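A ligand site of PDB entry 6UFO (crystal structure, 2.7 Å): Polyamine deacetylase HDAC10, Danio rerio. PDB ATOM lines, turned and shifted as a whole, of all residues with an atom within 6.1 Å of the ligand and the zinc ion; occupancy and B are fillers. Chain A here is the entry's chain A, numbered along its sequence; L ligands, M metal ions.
OD2 of Asp 94 is in salt-bridge range of N1 of the ligand (3.0 Å).
O3 of the ligand lies close to NE2 of His 137 (3.0 Å).
O2 of the ligand sits close to OH of Tyr 307 (2.7 Å).
NE2 of His 136 lies close to O3 of the ligand (3.1 Å).
ND1 of His 137 lies close to O of His 177 (3.2 Å).
NE1 of Trp 205 is in hydrogen-bond range of OD1 of Asn 93, 2.5 Å away.
O of Asp 94 sits close to N of Gly 145.
SG of Cys 147 lies within hydrogen-bond range of N of His 137.
N of Gly 135 lies within hydrogen-bond range of SG of Cys 147, at 3.4 Å.
N of His 136 lies within hydrogen-bond range of SG of Cys 147, at 3.8 Å.
A ring nitrogen (NE2) of His 137 lies close to a ring nitrogen (NE2) of His 136 (3.1 Å).
O of Asp 94 sits at hydrogen-bond distance from N of Phe 146, 3.0 Å away.
Ala 24 touches the ligand (CB to C5, 3.7 Å).
Pro 134 touches the ligand (CB to O1, 3.4 Å).
O of Gly 145 touches C9 of the ligand, 3.4 Å away.
Phe 146 touches the ligand.
Cys 147 touches the ligand (SG to O1, 3.96 Å).
Trp 205 touches the ligand (CZ3 to C1, 3.6 Å).
Glu 274 touches the ligand (OE1 to C3, 3.3 Å).
Glu 304 touches the ligand.
Gly 305 touches the ligand (CA to C7, 3.6 Å).
Hydrophobic or aromatic side chains that line the ligand: Ala 24, Pro 134, His 136, His 137, Phe 146, His 176, Trp 205 and Tyr 307.
Within 4 Å of the ligand: Ala 24, Asp 94, Pro 134, His 136, His 137, Gly 145, Phe 146, Cys 147, Asp 174, His 176, Trp 205, Asp 267, Glu 274, Glu 304, Gly 305 and Tyr 307.
The zinc ion is bound by OD2 of Asp 267 (2.0 Å), O2 of the ligand (2.0 Å), OD2 of Asp 174 (2.1 Å), ND1 of His 176 (2.2 Å), O3 of the ligand (2.2 Å) and OD1 of Asp 174 (2.5 Å).
The zinc ion has six donor atoms within binding distance.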
ATOM      1  N   ALA A  24      13.447   1.766 -17.328  1.00  0.00           N
ATOM      2  CA  ALA A  24      13.035   2.574 -16.191  1.00  0.00           C
ATOM      3  C   ALA A  24      11.579   2.367 -15.799  1.00  0.00           C
ATOM      4  O   ALA A  24      11.172   2.844 -14.735  1.00  0.00           O
ATOM      5  CB  ALA A  24      13.277   4.055 -16.484  1.00  0.00           C
ATOM      6  N   CYS A  25      10.789   1.679 -16.629  1.00  0.00           N
ATOM      7  CA  CYS A  25       9.362   1.515 -16.372  1.00  0.00           C
ATOM      8  C   CYS A  25       8.914   0.065 -16.241  1.00  0.00           C
ATOM      9  O   CYS A  25       7.778  -0.160 -15.807  1.00  0.00           O
ATOM     10  CB  CYS A  25       8.545   2.181 -17.495  1.00  0.00           C
ATOM     11  SG  CYS A  25       8.479   3.989 -17.416  1.00  0.00           S
ATOM     12  N   ILE A  27       9.376  -2.130 -14.151  1.00  0.00           N
ATOM     13  CA  ILE A  27       9.100  -2.632 -12.800  1.00  0.00           C
ATOM     14  C   ILE A  27       7.668  -2.350 -12.357  1.00  0.00           C
ATOM     15  O   ILE A  27       7.212  -2.936 -11.381  1.00  0.00           O
ATOM     16  CB  ILE A  27      10.076  -2.030 -11.777  1.00  0.00           C
ATOM     17  CG1 ILE A  27      10.054  -0.507 -11.843  1.00  0.00           C
ATOM     18  CG2 ILE A  27      11.479  -2.573 -11.999  1.00  0.00           C
ATOM     19  CD1 ILE A  27      10.519   0.170 -10.574  1.00  0.00           C
ATOM     20  N   ASN A  93       8.578  12.365 -17.874  1.00  0.00           N
ATOM     21  CA  ASN A  93       9.734  11.707 -17.271  1.00  0.00           C
ATOM     22  C   ASN A  93       9.286  10.415 -16.583  1.00  0.00           C
ATOM     23  O   ASN A  93       8.546  10.448 -15.601  1.00  0.00           O
ATOM     24  CB  ASN A  93      10.423  12.637 -16.281  1.00  0.00           C
ATOM     25  CG  ASN A  93      11.764  12.091 -15.802  1.00  0.00           C
ATOM     26  OD1 ASN A  93      11.897  11.675 -14.657  1.00  0.00           O
ATOM     27  ND2 ASN A  93      12.745  12.099 -16.688  1.00  0.00           N
ATOM     28  N   ASP A  94       9.754   9.277 -17.107  1.00  0.00           N
ATOM     29  CA  ASP A  94       9.568   7.962 -16.503  1.00  0.00           C
ATOM     30  C   ASP A  94       8.093   7.624 -16.297  1.00  0.00           C
ATOM     31  O   ASP A  94       7.625   7.391 -15.179  1.00  0.00           O
ATOM     32  CB  ASP A  94      10.351   7.860 -15.185  1.00  0.00           C
ATOM     33  CG  ASP A  94      11.846   7.720 -15.402  1.00  0.00           C
ATOM     34  OD1 ASP A  94      12.267   7.600 -16.574  1.00  0.00           O
ATOM     35  OD2 ASP A  94      12.597   7.712 -14.409  1.00  0.00           O
ATOM     36  N   PRO A 134      -0.200   4.886  -9.565  1.00  0.00           N
ATOM     37  CA  PRO A 134       0.009   5.765  -8.403  1.00  0.00           C
ATOM     38  C   PRO A 134      -0.164   7.231  -8.757  1.00  0.00           C
ATOM     39  O   PRO A 134      -0.504   7.555  -9.892  1.00  0.00           O
ATOM     40  CB  PRO A 134       1.444   5.435  -7.984  1.00  0.00           C
ATOM     41  CG  PRO A 134       2.103   4.982  -9.236  1.00  0.00           C
ATOM     42  CD  PRO A 134       1.045   4.225  -9.992  1.00  0.00           C
ATOM     43  N   GLY A 135       0.082   8.128  -7.799  1.00  0.00           N
ATOM     44  CA  GLY A 135      -0.247   9.521  -8.048  1.00  0.00           C
ATOM     45  C   GLY A 135       0.682  10.598  -7.515  1.00  0.00           C
ATOM     46  O   GLY A 135       0.712  11.696  -8.074  1.00  0.00           O
ATOM     47  N   HIS A 136       1.446  10.306  -6.457  1.00  0.00           N
ATOM     48  CA  HIS A 136       2.092  11.398  -5.718  1.00  0.00           C
ATOM     49  C   HIS A 136       3.164  12.131  -6.522  1.00  0.00           C
ATOM     50  O   HIS A 136       3.635  13.168  -6.071  1.00  0.00           O
ATOM     51  CB  HIS A 136       2.654  10.871  -4.389  1.00  0.00           C
ATOM     52  CG  HIS A 136       3.939  10.115  -4.497  1.00  0.00           C
ATOM     53  ND1 HIS A 136       4.643   9.703  -3.383  1.00  0.00           N
ATOM     54  CD2 HIS A 136       4.653   9.698  -5.567  1.00  0.00           C
ATOM     55  CE1 HIS A 136       5.734   9.059  -3.766  1.00  0.00           C
ATOM     56  NE2 HIS A 136       5.764   9.041  -5.089  1.00  0.00           N
ATOM     57  N   HIS A 137       3.544  11.617  -7.700  1.00  0.00           N
ATOM     58  CA  HIS A 137       4.456  12.337  -8.579  1.00  0.00           C
ATOM     59  C   HIS A 137       3.738  13.209  -9.588  1.00  0.00           C
ATOM     60  O   HIS A 137       4.376  14.063 -10.219  1.00  0.00           O
ATOM     61  CB  HIS A 137       5.361  11.347  -9.334  1.00  0.00           C
ATOM     62  CG  HIS A 137       6.365  10.655  -8.459  1.00  0.00           C
ATOM     63  ND1 HIS A 137       7.045  11.295  -7.451  1.00  0.00           N
ATOM     64  CD2 HIS A 137       6.810   9.378  -8.459  1.00  0.00           C
ATOM     65  CE1 HIS A 137       7.859  10.444  -6.866  1.00  0.00           C
ATOM     66  NE2 HIS A 137       7.744   9.273  -7.458  1.00  0.00           N
ATOM     67  N   GLY A 145       6.743   9.809 -13.148  1.00  0.00           N
ATOM     68  CA  GLY A 145       7.028   8.657 -12.314  1.00  0.00           C
ATOM     69  C   GLY A 145       5.880   7.686 -12.138  1.00  0.00           C
ATOM     70  O   GLY A 145       5.432   7.445 -11.008  1.00  0.00           O
ATOM     71  N   PHE A 146       5.384   7.145 -13.253  1.00  0.00           N
ATOM     72  CA  PHE A 146       4.275   6.185 -13.310  1.00  0.00           C
ATOM     73  C   PHE A 146       2.945   6.777 -12.883  1.00  0.00           C
ATOM     74  O   PHE A 146       1.948   6.051 -12.799  1.00  0.00           O
ATOM     75  CB  PHE A 146       4.543   4.937 -12.449  1.00  0.00           C
ATOM     76  CG  PHE A 146       5.901   4.320 -12.651  1.00  0.00           C
ATOM     77  CD1 PHE A 146       6.546   4.389 -13.875  1.00  0.00           C
ATOM     78  CD2 PHE A 146       6.528   3.658 -11.597  1.00  0.00           C
ATOM     79  CE1 PHE A 146       7.796   3.827 -14.045  1.00  0.00           C
ATOM     80  CE2 PHE A 146       7.773   3.090 -11.773  1.00  0.00           C
ATOM     81  CZ  PHE A 146       8.406   3.167 -12.996  1.00  0.00           C
ATOM     82  N   CYS A 147       2.889   8.078 -12.607  1.00  0.00           N
ATOM     83  CA  CYS A 147       1.686   8.723 -12.088  1.00  0.00           C
ATOM     84  C   CYS A 147       1.025   9.565 -13.168  1.00  0.00           C
ATOM     85  O   CYS A 147       1.699  10.314 -13.884  1.00  0.00           O
ATOM     86  CB  CYS A 147       2.010   9.591 -10.872  1.00  0.00           C
ATOM     87  SG  CYS A 147       2.903   8.737  -9.567  1.00  0.00           S
ATOM     88  N   ASP A 174       6.435   6.503   1.031  1.00  0.00           N
ATOM     89  CA  ASP A 174       7.023   5.953  -0.182  1.00  0.00           C
ATOM     90  C   ASP A 174       8.503   6.330  -0.238  1.00  0.00           C
ATOM     91  O   ASP A 174       8.929   7.340   0.324  1.00  0.00           O
ATOM     92  CB  ASP A 174       6.287   6.479  -1.408  1.00  0.00           C
ATOM     93  CG  ASP A 174       6.791   5.885  -2.710  1.00  0.00           C
ATOM     94  OD1 ASP A 174       6.205   4.894  -3.187  1.00  0.00           O
ATOM     95  OD2 ASP A 174       7.764   6.429  -3.262  1.00  0.00           O
ATOM     96  N   VAL A 175       9.304   5.509  -0.925  1.00  0.00           N
ATOM     97  CA  VAL A 175      10.737   5.750  -0.971  1.00  0.00           C
ATOM     98  C   VAL A 175      11.103   6.909  -1.895  1.00  0.00           C
ATOM     99  O   VAL A 175      12.236   7.397  -1.828  1.00  0.00           O
ATOM    100  CB  VAL A 175      11.502   4.477  -1.397  1.00  0.00           C
ATOM    101  CG1 VAL A 175      11.573   4.363  -2.916  1.00  0.00           C
ATOM    102  CG2 VAL A 175      12.891   4.463  -0.777  1.00  0.00           C
ATOM    103  N   HIS A 176      10.188   7.350  -2.744  1.00  0.00           N
ATOM    104  CA  HIS A 176      10.412   8.505  -3.606  1.00  0.00           C
ATOM    105  C   HIS A 176       9.725   9.738  -3.019  1.00  0.00           C
ATOM    106  O   HIS A 176       8.750   9.633  -2.275  1.00  0.00           O
ATOM    107  CB  HIS A 176       9.876   8.251  -5.021  1.00  0.00           C
ATOM    108  CG  HIS A 176      10.496   7.072  -5.688  1.00  0.00           C
ATOM    109  ND1 HIS A 176      10.033   5.781  -5.520  1.00  0.00           N
ATOM    110  CD2 HIS A 176      11.529   6.983  -6.556  1.00  0.00           C
ATOM    111  CE1 HIS A 176      10.763   4.960  -6.234  1.00  0.00           C
ATOM    112  NE2 HIS A 176      11.688   5.656  -6.875  1.00  0.00           N
ATOM    113  N   HIS A 177      10.260  10.903  -3.371  1.00  0.00           N
ATOM    114  CA  HIS A 177       9.679  12.164  -2.916  1.00  0.00           C
ATOM    115  C   HIS A 177       8.452  12.489  -3.757  1.00  0.00           C
ATOM    116  O   HIS A 177       8.547  12.594  -4.982  1.00  0.00           O
ATOM    117  CB  HIS A 177      10.703  13.299  -2.999  1.00  0.00           C
ATOM    118  CG  HIS A 177      10.152  14.627  -2.599  1.00  0.00           C
ATOM    119  ND1 HIS A 177      10.281  15.758  -3.382  1.00  0.00           N
ATOM    120  CD2 HIS A 177       9.474  15.020  -1.495  1.00  0.00           C
ATOM    121  CE1 HIS A 177       9.709  16.787  -2.776  1.00  0.00           C
ATOM    122  NE2 HIS A 177       9.213  16.359  -1.629  1.00  0.00           N
ATOM    123  N   TRP A 205      16.594   9.814  -8.260  1.00  0.00           N
ATOM    124  CA  TRP A 205      15.418  10.337  -8.935  1.00  0.00           C
ATOM    125  C   TRP A 205      14.389  10.815  -7.909  1.00  0.00           C
ATOM    126  O   TRP A 205      14.199  10.159  -6.870  1.00  0.00           O
ATOM    127  CB  TRP A 205      14.814   9.258  -9.837  1.00  0.00           C
ATOM    128  CG  TRP A 205      13.799   9.757 -10.811  1.00  0.00           C
ATOM    129  CD1 TRP A 205      14.032  10.173 -12.088  1.00  0.00           C
ATOM    130  CD2 TRP A 205      12.401   9.909 -10.585  1.00  0.00           C
ATOM    131  NE1 TRP A 205      12.853  10.571 -12.679  1.00  0.00           N
ATOM    132  CE2 TRP A 205      11.832  10.411 -11.770  1.00  0.00           C
ATOM    133  CE3 TRP A 205      11.560   9.657  -9.489  1.00  0.00           C
ATOM    134  CZ2 TRP A 205      10.473  10.685 -11.895  1.00  0.00           C
ATOM    135  CZ3 TRP A 205      10.213   9.922  -9.615  1.00  0.00           C
ATOM    136  CH2 TRP A 205       9.673  10.429 -10.812  1.00  0.00           C
ATOM    137  N   GLY A 265       3.582   3.981  -0.105  1.00  0.00           N
ATOM    138  CA  GLY A 265       4.455   3.274  -1.017  1.00  0.00           C
ATOM    139  C   GLY A 265       5.369   2.340  -0.237  1.00  0.00           C
ATOM    140  O   GLY A 265       6.036   2.759   0.708  1.00  0.00           O
ATOM    141  N   ASP A 267       7.878   0.548  -1.538  1.00  0.00           N
ATOM    142  CA  ASP A 267       9.234   0.428  -2.058  1.00  0.00           C
ATOM    143  C   ASP A 267      10.287   0.872  -1.056  1.00  0.00           C
ATOM    144  O   ASP A 267      11.482   0.803  -1.364  1.00  0.00           O
ATOM    145  CB  ASP A 267       9.382   1.223  -3.359  1.00  0.00           C
ATOM    146  CG  ASP A 267       8.749   2.600  -3.274  1.00  0.00           C
ATOM    147  OD1 ASP A 267       8.310   2.996  -2.172  1.00  0.00           O
ATOM    148  OD2 ASP A 267       8.701   3.287  -4.318  1.00  0.00           O
ATOM    149  N   GLU A 274      14.145  -0.626  -6.169  1.00  0.00           N
ATOM    150  CA  GLU A 274      14.197   0.821  -6.373  1.00  0.00           C
ATOM    151  C   GLU A 274      14.540   1.582  -5.097  1.00  0.00           C
ATOM    152  O   GLU A 274      15.202   2.627  -5.179  1.00  0.00           O
ATOM    153  CB  GLU A 274      12.848   1.309  -6.921  1.00  0.00           C
ATOM    154  CG  GLU A 274      12.888   2.711  -7.500  1.00  0.00           C
ATOM    155  CD  GLU A 274      13.573   2.765  -8.852  1.00  0.00           C
ATOM    156  OE1 GLU A 274      14.100   3.846  -9.201  1.00  0.00           O
ATOM    157  OE2 GLU A 274      13.561   1.751  -9.566  1.00  0.00           O
ATOM    158  N   LEU A 303      -2.437   3.246  -1.774  1.00  0.00           N
ATOM    159  CA  LEU A 303      -1.274   2.535  -2.285  1.00  0.00           C
ATOM    160  C   LEU A 303      -0.528   3.389  -3.306  1.00  0.00           C
ATOM    161  O   LEU A 303      -1.134   4.062  -4.135  1.00  0.00           O
ATOM    162  CB  LEU A 303      -1.723   1.206  -2.908  1.00  0.00           C
ATOM    163  CG  LEU A 303      -0.710   0.142  -3.341  1.00  0.00           C
ATOM    164  CD1 LEU A 303      -0.272   0.340  -4.793  1.00  0.00           C
ATOM    165  CD2 LEU A 303       0.492   0.107  -2.414  1.00  0.00           C
ATOM    166  N   GLU A 304       0.806   3.359  -3.220  1.00  0.00           N
ATOM    167  CA  GLU A 304       1.642   4.142  -4.127  1.00  0.00           C
ATOM    168  C   GLU A 304       2.645   3.250  -4.836  1.00  0.00           C
ATOM    169  O   GLU A 304       2.355   2.702  -5.911  1.00  0.00           O
ATOM    170  CB  GLU A 304       2.360   5.248  -3.345  1.00  0.00           C
ATOM    171  CG  GLU A 304       1.438   6.314  -2.758  1.00  0.00           C
ATOM    172  CD  GLU A 304       1.025   7.389  -3.766  1.00  0.00           C
ATOM    173  OE1 GLU A 304       1.214   7.178  -4.980  1.00  0.00           O
ATOM    174  OE2 GLU A 304       0.507   8.436  -3.342  1.00  0.00           O
ATOM    175  N   GLY A 305       3.835   3.085  -4.251  1.00  0.00           N
ATOM    176  CA  GLY A 305       4.878   2.256  -4.819  1.00  0.00           C
ATOM    177  C   GLY A 305       4.998   0.904  -4.136  1.00  0.00           C
ATOM    178  O   GLY A 305       4.184   0.515  -3.298  1.00  0.00           O
ATOM    179  N   GLY A 306       6.058   0.193  -4.499  1.00  0.00           N
ATOM    180  CA  GLY A 306       6.300  -1.155  -4.006  1.00  0.00           C
ATOM    181  C   GLY A 306       6.438  -2.147  -5.141  1.00  0.00           C
ATOM    182  O   GLY A 306       5.447  -2.489  -5.795  1.00  0.00           O
ATOM    183  N   TYR A 307       7.665  -2.631  -5.388  1.00  0.00           N
ATOM    184  CA  TYR A 307       7.958  -3.385  -6.592  1.00  0.00           C
ATOM    185  C   TYR A 307       8.537  -4.769  -6.362  1.00  0.00           C
ATOM    186  O   TYR A 307       8.706  -5.518  -7.332  1.00  0.00           O
ATOM    187  CB  TYR A 307       8.899  -2.577  -7.497  1.00  0.00           C
ATOM    188  CG  TYR A 307       8.393  -1.187  -7.763  1.00  0.00           C
ATOM    189  CD1 TYR A 307       7.395  -0.967  -8.702  1.00  0.00           C
ATOM    190  CD2 TYR A 307       8.885  -0.102  -7.060  1.00  0.00           C
ATOM    191  CE1 TYR A 307       6.913   0.300  -8.949  1.00  0.00           C
ATOM    192  CE2 TYR A 307       8.413   1.178  -7.297  1.00  0.00           C
ATOM    193  CZ  TYR A 307       7.420   1.369  -8.240  1.00  0.00           C
ATOM    194  OH  TYR A 307       6.941   2.628  -8.482  1.00  0.00           O
HETATM  195  C1  LIG L   1      10.223   6.592 -10.931  1.00  0.00           C
HETATM  196  C2  LIG L   1      11.712   6.116 -10.949  1.00  0.00           C
HETATM  197  C3  LIG L   1      13.398   4.815 -12.254  1.00  0.00           C
HETATM  198  C4  LIG L   1      14.716   5.634 -12.397  1.00  0.00           C
HETATM  199  C5  LIG L   1      15.376   5.547 -13.808  1.00  0.00           C
HETATM  200  C6  LIG L   1       4.073   6.515  -6.071  1.00  0.00           C
HETATM  201  C7  LIG L   1       5.515   4.980  -7.009  1.00  0.00           C
HETATM  202  C8  LIG L   1       7.029   5.454  -7.069  1.00  0.00           C
HETATM  203  C9  LIG L   1       7.174   5.874  -8.546  1.00  0.00           C
HETATM  204  C10 LIG L   1       8.574   6.437  -8.887  1.00  0.00           C
HETATM  205  C11 LIG L   1       9.281   5.711 -10.065  1.00  0.00           C
HETATM  206  N1  LIG L   1      12.174   5.681 -12.300  1.00  0.00           N
HETATM  207  N2  LIG L   1      15.544   6.885 -14.424  1.00  0.00           N
HETATM  208  O1  LIG L   1       4.714   6.096  -7.237  1.00  0.00           O
HETATM  209  O2  LIG L   1       7.858   4.410  -6.700  1.00  0.00           O
HETATM  210  O3  LIG L   1       7.243   6.564  -6.254  1.00  0.00           O
HETATM  211 ZN    ZN M   1       8.086   5.086  -4.829  1.00  0.00          ZN
